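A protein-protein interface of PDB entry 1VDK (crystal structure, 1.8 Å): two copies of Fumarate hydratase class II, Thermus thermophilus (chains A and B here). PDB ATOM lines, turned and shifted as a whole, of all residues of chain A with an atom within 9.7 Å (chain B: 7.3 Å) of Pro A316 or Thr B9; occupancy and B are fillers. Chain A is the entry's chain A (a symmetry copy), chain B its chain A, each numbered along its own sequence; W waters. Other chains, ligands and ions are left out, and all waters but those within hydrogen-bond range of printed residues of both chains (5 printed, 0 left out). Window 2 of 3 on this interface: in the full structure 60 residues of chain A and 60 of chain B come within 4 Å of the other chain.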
ATOM      1  N   PRO A 312      26.458  17.383  -7.907  1.00  0.00           N
ATOM      2  CA  PRO A 312      25.594  18.542  -8.159  1.00  0.00           C
ATOM      3  C   PRO A 312      24.762  18.950  -6.941  1.00  0.00           C
ATOM      4  O   PRO A 312      24.274  18.096  -6.199  1.00  0.00           O
ATOM      5  CB  PRO A 312      24.703  18.067  -9.305  1.00  0.00           C
ATOM      6  CG  PRO A 312      25.559  17.072 -10.020  1.00  0.00           C
ATOM      7  CD  PRO A 312      26.183  16.311  -8.880  1.00  0.00           C
ATOM      8  N   ALA A 313      24.604  20.256  -6.748  1.00  0.00           N
ATOM      9  CA  ALA A 313      23.808  20.792  -5.647  1.00  0.00           C
ATOM     10  C   ALA A 313      22.459  21.188  -6.244  1.00  0.00           C
ATOM     11  O   ALA A 313      22.372  22.155  -7.001  1.00  0.00           O
ATOM     12  CB  ALA A 313      24.499  22.012  -5.043  1.00  0.00           C
ATOM     13  N   ASN A 314      21.409  20.445  -5.902  1.00  0.00           N
ATOM     14  CA  ASN A 314      20.081  20.710  -6.452  1.00  0.00           C
ATOM     15  C   ASN A 314      19.131  21.511  -5.574  1.00  0.00           C
ATOM     16  O   ASN A 314      18.106  21.997  -6.056  1.00  0.00           O
ATOM     17  CB  ASN A 314      19.415  19.390  -6.835  1.00  0.00           C
ATOM     18  CG  ASN A 314      20.273  18.558  -7.758  1.00  0.00           C
ATOM     19  OD1 ASN A 314      20.714  19.034  -8.805  1.00  0.00           O
ATOM     20  ND2 ASN A 314      20.520  17.309  -7.379  1.00  0.00           N
ATOM     21  N   GLU A 315      19.449  21.637  -4.290  1.00  0.00           N
ATOM     22  CA  GLU A 315      18.597  22.405  -3.390  1.00  0.00           C
ATOM     23  C   GLU A 315      19.394  23.062  -2.261  1.00  0.00           C
ATOM     24  O   GLU A 315      20.544  22.700  -2.008  1.00  0.00           O
ATOM     25  CB  GLU A 315      17.473  21.522  -2.819  1.00  0.00           C
ATOM     26  CG  GLU A 315      17.890  20.415  -1.852  1.00  0.00           C
ATOM     27  CD  GLU A 315      18.340  19.135  -2.541  1.00  0.00           C
ATOM     28  OE1 GLU A 315      17.741  18.762  -3.574  1.00  0.00           O
ATOM     29  OE2 GLU A 315      19.283  18.491  -2.032  1.00  0.00           O
ATOM     30  N   PRO A 316      18.797  24.059  -1.582  1.00  0.00           N
ATOM     31  CA  PRO A 316      19.451  24.772  -0.479  1.00  0.00           C
ATOM     32  C   PRO A 316      19.926  23.878   0.670  1.00  0.00           C
ATOM     33  O   PRO A 316      21.090  23.935   1.072  1.00  0.00           O
ATOM     34  CB  PRO A 316      18.378  25.760  -0.024  1.00  0.00           C
ATOM     35  CG  PRO A 316      17.641  26.053  -1.284  1.00  0.00           C
ATOM     36  CD  PRO A 316      17.498  24.679  -1.901  1.00  0.00           C
ATOM     37  N   GLY A 317      19.021  23.060   1.198  1.00  0.00           N
ATOM     38  CA  GLY A 317      19.372  22.189   2.305  1.00  0.00           C
ATOM     39  C   GLY A 317      19.004  22.835   3.629  1.00  0.00           C
ATOM     40  O   GLY A 317      18.627  24.008   3.663  1.00  0.00           O
ATOM     41  N   SER A 318      19.108  22.082   4.721  1.00  0.00           N
ATOM     42  CA  SER A 318      18.769  22.614   6.038  1.00  0.00           C
ATOM     43  C   SER A 318      19.837  23.577   6.558  1.00  0.00           C
ATOM     44  O   SER A 318      19.596  24.782   6.662  1.00  0.00           O
ATOM     45  CB  SER A 318      18.552  21.468   7.034  1.00  0.00           C
ATOM     46  OG  SER A 318      19.676  20.610   7.101  1.00  0.00           O
ATOM     47  N   SER A 319      21.013  23.049   6.884  1.00  0.00           N
ATOM     48  CA  SER A 319      22.109  23.876   7.378  1.00  0.00           C
ATOM     49  C   SER A 319      22.977  24.304   6.199  1.00  0.00           C
ATOM     50  O   SER A 319      23.455  23.465   5.434  1.00  0.00           O
ATOM     51  CB  SER A 319      22.955  23.097   8.388  1.00  0.00           C
ATOM     52  OG  SER A 319      23.534  21.950   7.791  1.00  0.00           O
ATOM     53  N   ILE A 320      23.181  25.609   6.056  1.00  0.00           N
ATOM     54  CA  ILE A 320      23.977  26.136   4.954  1.00  0.00           C
ATOM     55  C   ILE A 320      25.454  26.331   5.288  1.00  0.00           C
ATOM     56  O   ILE A 320      25.807  26.854   6.343  1.00  0.00           O
ATOM     57  CB  ILE A 320      23.408  27.487   4.456  1.00  0.00           C
ATOM     58  CG1 ILE A 320      21.977  27.294   3.946  1.00  0.00           C
ATOM     59  CG2 ILE A 320      24.291  28.055   3.354  1.00  0.00           C
ATOM     60  CD1 ILE A 320      21.855  26.327   2.782  1.00  0.00           C
ATOM     61  N   MET A 321      26.305  25.894   4.365  1.00  0.00           N
ATOM     62  CA  MET A 321      27.753  26.019   4.489  1.00  0.00           C
ATOM     63  C   MET A 321      28.305  26.068   3.070  1.00  0.00           C
ATOM     64  O   MET A 321      28.036  25.177   2.264  1.00  0.00           O
ATOM     65  CB  MET A 321      28.357  24.817   5.223  1.00  0.00           C
ATOM     66  CG  MET A 321      29.882  24.876   5.323  1.00  0.00           C
ATOM     67  SD  MET A 321      30.654  23.360   5.938  1.00  0.00           S
ATOM     68  CE  MET A 321      30.561  23.621   7.713  1.00  0.00           C
ATOM     69  N   PRO A 322      29.076  27.114   2.744  1.00  0.00           N
ATOM     70  CA  PRO A 322      29.647  27.244   1.401  1.00  0.00           C
ATOM     71  C   PRO A 322      30.354  25.980   0.924  1.00  0.00           C
ATOM     72  O   PRO A 322      31.267  25.478   1.584  1.00  0.00           O
ATOM     73  CB  PRO A 322      30.604  28.422   1.552  1.00  0.00           C
ATOM     74  CG  PRO A 322      29.894  29.283   2.552  1.00  0.00           C
ATOM     75  CD  PRO A 322      29.445  28.268   3.583  1.00  0.00           C
ATOM     76  N   GLY A 323      29.916  25.463  -0.220  1.00  0.00           N
ATOM     77  CA  GLY A 323      30.528  24.272  -0.777  1.00  0.00           C
ATOM     78  C   GLY A 323      29.932  22.950  -0.333  1.00  0.00           C
ATOM     79  O   GLY A 323      30.139  21.933  -0.995  1.00  0.00           O
ATOM     80  N   LYS A 324      29.201  22.944   0.780  1.00  0.00           N
ATOM     81  CA  LYS A 324      28.604  21.704   1.270  1.00  0.00           C
ATOM     82  C   LYS A 324      27.343  21.321   0.510  1.00  0.00           C
ATOM     83  O   LYS A 324      26.426  22.127   0.361  1.00  0.00           O
ATOM     84  CB  LYS A 324      28.251  21.803   2.755  1.00  0.00           C
ATOM     85  CG  LYS A 324      27.715  20.485   3.303  1.00  0.00           C
ATOM     86  CD  LYS A 324      26.520  20.666   4.228  1.00  0.00           C
ATOM     87  CE  LYS A 324      26.899  21.369   5.513  1.00  0.00           C
ATOM     88  NZ  LYS A 324      25.779  21.333   6.493  1.00  0.00           N
ATOM     89  N   VAL A 325      27.301  20.076   0.048  1.00  0.00           N
ATOM     90  CA  VAL A 325      26.158  19.562  -0.692  1.00  0.00           C
ATOM     91  C   VAL A 325      25.735  18.221  -0.096  1.00  0.00           C
ATOM     92  O   VAL A 325      26.475  17.241  -0.191  1.00  0.00           O
ATOM     93  CB  VAL A 325      26.515  19.341  -2.181  1.00  0.00           C
ATOM     94  CG1 VAL A 325      25.311  18.794  -2.936  1.00  0.00           C
ATOM     95  CG2 VAL A 325      26.991  20.648  -2.804  1.00  0.00           C
ATOM     96  N   ASN A 326      24.561  18.174   0.530  1.00  0.00           N
ATOM     97  CA  ASN A 326      24.091  16.913   1.094  1.00  0.00           C
ATOM     98  C   ASN A 326      23.751  15.988  -0.073  1.00  0.00           C
ATOM     99  O   ASN A 326      23.161  16.419  -1.058  1.00  0.00           O
ATOM    100  CB  ASN A 326      22.847  17.120   1.971  1.00  0.00           C
ATOM    101  CG  ASN A 326      23.164  17.819   3.285  1.00  0.00           C
ATOM    102  OD1 ASN A 326      24.285  17.739   3.791  1.00  0.00           O
ATOM    103  ND2 ASN A 326      22.167  18.492   3.854  1.00  0.00           N
ATOM    104  N   THR A 328      21.490  14.183  -1.159  1.00  0.00           N
ATOM    105  CA  THR A 328      20.071  13.876  -1.100  1.00  0.00           C
ATOM    106  C   THR A 328      19.570  12.793  -2.055  1.00  0.00           C
ATOM    107  O   THR A 328      18.699  12.006  -1.684  1.00  0.00           O
ATOM    108  CB  THR A 328      19.241  15.168  -1.263  1.00  0.00           C
ATOM    109  OG1 THR A 328      19.549  15.791  -2.510  1.00  0.00           O
ATOM    110  CG2 THR A 328      19.578  16.137  -0.145  1.00  0.00           C
ATOM    111  N   ARG B   7      11.196  32.404  -3.273  1.00  0.00           N
ATOM    112  CA  ARG B   7      12.648  32.326  -3.278  1.00  0.00           C
ATOM    113  C   ARG B   7      13.246  31.681  -2.038  1.00  0.00           C
ATOM    114  O   ARG B   7      12.638  31.662  -0.970  1.00  0.00           O
ATOM    115  CB  ARG B   7      13.241  33.730  -3.412  1.00  0.00           C
ATOM    116  CG  ARG B   7      12.966  34.621  -2.205  1.00  0.00           C
ATOM    117  CD  ARG B   7      13.724  35.941  -2.298  1.00  0.00           C
ATOM    118  NE  ARG B   7      13.536  36.770  -1.109  1.00  0.00           N
ATOM    119  CZ  ARG B   7      12.376  37.303  -0.740  1.00  0.00           C
ATOM    120  NH1 ARG B   7      11.285  37.099  -1.467  1.00  0.00           N
ATOM    121  NH2 ARG B   7      12.306  38.046   0.355  1.00  0.00           N
ATOM    122  N   ASP B   8      14.449  31.146  -2.209  1.00  0.00           N
ATOM    123  CA  ASP B   8      15.211  30.549  -1.122  1.00  0.00           C
ATOM    124  C   ASP B   8      16.649  30.979  -1.382  1.00  0.00           C
ATOM    125  O   ASP B   8      16.910  31.696  -2.351  1.00  0.00           O
ATOM    126  CB  ASP B   8      15.084  29.016  -1.096  1.00  0.00           C
ATOM    127  CG  ASP B   8      15.453  28.361  -2.413  1.00  0.00           C
ATOM    128  OD1 ASP B   8      16.370  28.858  -3.103  1.00  0.00           O
ATOM    129  OD2 ASP B   8      14.832  27.324  -2.743  1.00  0.00           O
ATOM    130  N   THR B   9      17.577  30.556  -0.536  1.00  0.00           N
ATOM    131  CA  THR B   9      18.972  30.949  -0.699  1.00  0.00           C
ATOM    132  C   THR B   9      19.571  30.605  -2.062  1.00  0.00           C
ATOM    133  O   THR B   9      20.572  31.196  -2.468  1.00  0.00           O
ATOM    134  CB  THR B   9      19.858  30.321   0.394  1.00  0.00           C
ATOM    135  OG1 THR B   9      19.746  28.894   0.341  1.00  0.00           O
ATOM    136  CG2 THR B   9      19.425  30.811   1.768  1.00  0.00           C
ATOM    137  N   MET B  10      18.957  29.664  -2.770  1.00  0.00           N
ATOM    138  CA  MET B  10      19.463  29.255  -4.075  1.00  0.00           C
ATOM    139  C   MET B  10      18.920  30.110  -5.218  1.00  0.00           C
ATOM    140  O   MET B  10      19.522  30.173  -6.291  1.00  0.00           O
ATOM    141  CB  MET B  10      19.133  27.781  -4.323  1.00  0.00           C
ATOM    142  CG  MET B  10      19.785  27.194  -5.565  1.00  0.00           C
ATOM    143  SD  MET B  10      19.556  25.404  -5.663  1.00  0.00           S
ATOM    144  CE  MET B  10      20.858  24.845  -4.580  1.00  0.00           C
ATOM    145  N   GLY B  11      17.787  30.765  -4.993  1.00  0.00           N
ATOM    146  CA  GLY B  11      17.218  31.606  -6.032  1.00  0.00           C
ATOM    147  C   GLY B  11      15.703  31.628  -6.051  1.00  0.00           C
ATOM    148  O   GLY B  11      15.050  31.178  -5.110  1.00  0.00           O
ATOM    149  N   GLU B  12      15.140  32.157  -7.133  1.00  0.00           N
ATOM    150  CA  GLU B  12      13.693  32.243  -7.275  1.00  0.00           C
ATOM    151  C   GLU B  12      13.131  31.141  -8.166  1.00  0.00           C
ATOM    152  O   GLU B  12      13.783  30.694  -9.111  1.00  0.00           O
ATOM    153  CB  GLU B  12      13.300  33.620  -7.828  1.00  0.00           C
ATOM    154  CG  GLU B  12      13.367  34.730  -6.786  1.00  0.00           C
ATOM    155  CD  GLU B  12      12.964  36.089  -7.331  1.00  0.00           C
ATOM    156  OE1 GLU B  12      12.625  36.975  -6.518  1.00  0.00           O
ATOM    157  OE2 GLU B  12      12.994  36.275  -8.566  1.00  0.00           O
ATOM    158  N   ALA B  23       9.576  27.951  -2.224  1.00  0.00           N
ATOM    159  CA  ALA B  23      10.636  27.500  -3.118  1.00  0.00           C
ATOM    160  C   ALA B  23      11.225  26.124  -2.838  1.00  0.00           C
ATOM    161  O   ALA B  23      11.411  25.332  -3.759  1.00  0.00           O
ATOM    162  CB  ALA B  23      11.757  28.538  -3.149  1.00  0.00           C
ATOM    163  N   GLN B  24      11.530  25.830  -1.580  1.00  0.00           N
ATOM    164  CA  GLN B  24      12.128  24.541  -1.273  1.00  0.00           C
ATOM    165  C   GLN B  24      11.147  23.388  -1.458  1.00  0.00           C
ATOM    166  O   GLN B  24      11.553  22.262  -1.744  1.00  0.00           O
ATOM    167  CB  GLN B  24      12.742  24.574   0.130  1.00  0.00           C
ATOM    168  CG  GLN B  24      13.874  25.601   0.200  1.00  0.00           C
ATOM    169  CD  GLN B  24      14.568  25.666   1.543  1.00  0.00           C
ATOM    170  OE1 GLN B  24      15.213  24.709   1.973  1.00  0.00           O
ATOM    171  NE2 GLN B  24      14.446  26.807   2.211  1.00  0.00           N
ATOM    172  N   ARG B  27      11.156  22.807  -5.288  1.00  0.00           N
ATOM    173  CA  ARG B  27      12.344  22.096  -5.744  1.00  0.00           C
ATOM    174  C   ARG B  27      12.205  20.607  -5.433  1.00  0.00           C
ATOM    175  O   ARG B  27      12.471  19.760  -6.282  1.00  0.00           O
ATOM    176  CB  ARG B  27      13.606  22.649  -5.072  1.00  0.00           C
ATOM    177  CG  ARG B  27      13.958  24.089  -5.454  1.00  0.00           C
ATOM    178  CD  ARG B  27      15.312  24.486  -4.865  1.00  0.00           C
ATOM    179  NE  ARG B  27      15.563  25.927  -4.930  1.00  0.00           N
ATOM    180  CZ  ARG B  27      15.869  26.595  -6.039  1.00  0.00           C
ATOM    181  NH1 ARG B  27      15.971  25.958  -7.199  1.00  0.00           N
ATOM    182  NH2 ARG B  27      16.070  27.907  -5.987  1.00  0.00           N
ATOM    183  N   THR B 101      14.079  17.235   5.593  1.00  0.00           N
ATOM    184  CA  THR B 101      14.254  18.682   5.450  1.00  0.00           C
ATOM    185  C   THR B 101      13.224  19.328   4.532  1.00  0.00           C
ATOM    186  O   THR B 101      12.713  20.412   4.821  1.00  0.00           O
ATOM    187  CB  THR B 101      15.649  19.018   4.887  1.00  0.00           C
ATOM    188  OG1 THR B 101      16.649  18.656   5.844  1.00  0.00           O
ATOM    189  CG2 THR B 101      15.761  20.517   4.573  1.00  0.00           C
ATOM    190  N   LYS B 126       6.934  36.869   2.961  1.00  0.00           N
ATOM    191  CA  LYS B 126       7.709  36.345   4.075  1.00  0.00           C
ATOM    192  C   LYS B 126       7.702  37.278   5.288  1.00  0.00           C
ATOM    193  O   LYS B 126       8.661  37.294   6.061  1.00  0.00           O
ATOM    194  CB  LYS B 126       9.157  36.069   3.644  1.00  0.00           C
ATOM    195  CG  LYS B 126       9.314  34.930   2.639  1.00  0.00           C
ATOM    196  CD  LYS B 126      10.784  34.635   2.373  1.00  0.00           C
ATOM    197  CE  LYS B 126      10.962  33.413   1.487  1.00  0.00           C
ATOM    198  NZ  LYS B 126      12.397  33.061   1.315  1.00  0.00           N
ATOM    199  N   ASN B 131      11.944  30.451   7.709  1.00  0.00           N
ATOM    200  CA  ASN B 131      13.136  30.100   8.470  1.00  0.00           C
ATOM    201  C   ASN B 131      13.365  30.942   9.719  1.00  0.00           C
ATOM    202  O   ASN B 131      13.621  30.403  10.790  1.00  0.00           O
ATOM    203  CB  ASN B 131      14.377  30.179   7.573  1.00  0.00           C
ATOM    204  CG  ASN B 131      14.563  28.934   6.719  1.00  0.00           C
ATOM    205  OD1 ASN B 131      15.181  28.983   5.655  1.00  0.00           O
ATOM    206  ND2 ASN B 131      14.042  27.807   7.193  1.00  0.00           N
HETATM  207  O   HOH W   1      19.221  17.929   7.445  1.00  0.00           O
HETATM  208  O   HOH W   2      16.065  23.135  -8.027  1.00  0.00           O
HETATM  209  O   HOH W   3      15.978  22.107   0.601  1.00  0.00           O
HETATM  210  O   HOH W   4      16.333  25.246   7.158  1.00  0.00           O
HETATM  211  O   HOH W   5      16.652  25.934   4.532  1.00  0.00           O
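O of Asn A314 sits close to SD of Met B10 (3.7 Å).
Water W1 bridges the side-chain hydroxyl of Ser A318 (2.7 Å) and the side-chain hydroxyl of Thr B101 (3.1 Å).
Water W5 bridges O of Gly A317 and OE1 of Gln B24.
Water W2 lies within hydrogen-bond range of NH1 of Arg B27 (2.9 Å) and O of Asn A314 (3.1 Å).
Water W3 lies within hydrogen-bond range of the side-chain amide oxygen (OE1) of Gln B24 (3.0 Å) and the backbone NH (N) of Gly A317 (3.2 Å).
Water W4 bridges O of Ser A318 (3.3 Å) and ND2 of Asn B131 (3.4 Å).
Of chain B, only Asp B8, Thr B9, Met B10, Gln B24 and Arg B27 come within 4 Å of Pro A316.
No residue of chain A comes within 4 Å of Gly B11.
Printed residues of chain B within 4 Å of Ala A313: Met B10.
Of the printed residues of chain A, Gln B24 touches Pro A316 (3.9 Å) and Gly A317 (3.9 Å).
Of the printed residues of chain B, Asn A314 touches Met B10 (3.7 Å) and Arg B27 (3.9 Å).
Thr A328 touches none of the printed residues of chain B.
Met A321 touches none of the printed residues of chain B.
The nearest residue of chain B that does not touch Pro A316 is Gly B11 (6.0 Å).
The nearest printed residue of chain B that does not touch Ser A318 is Gln B24 (5.4 Å).
Hydrophobic or aromatic side chains of chain B that line the printed part of chain A: Met B10.
Among the printed residues, no Asp or Glu carboxylate lies within 4 Å of a Lys or Arg side-chain nitrogen of the other chain.
Among the printed residues, pairs that only touch across the chains: Glu A315 with Met B10, Pro A316 with Asp B8, Pro A316 with Thr B9, Ser A318 with Thr B101, Pro A316 with Arg B27, Pro A316 with Met B10, Gly A317 with Gln B24, Pro A316 with Gln B24, Ala A313 with Met B10 and Asn A314 with Arg B27.
OD1 of Asp B8 sits at hydrogen-bond distance from N of Met B10, at 2.7 Å.
OD1 of Asp B8 sits at hydrogen-bond distance from N of Gly B11, at 3.0 Å.
The guanidinium group (NE) of Arg B27 is in salt-bridge range of the side-chain carboxylate (OD2) of Asp B8, at 2.7 Å.
OE2 of Glu A315 sits at hydrogen-bond distance from OG1 of Thr A328 (2.8 Å).
No position is printed for both chains.
Of the 11 pairs that touch across the chains among the printed residues, none has its exchanged pair printed and touching as well.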
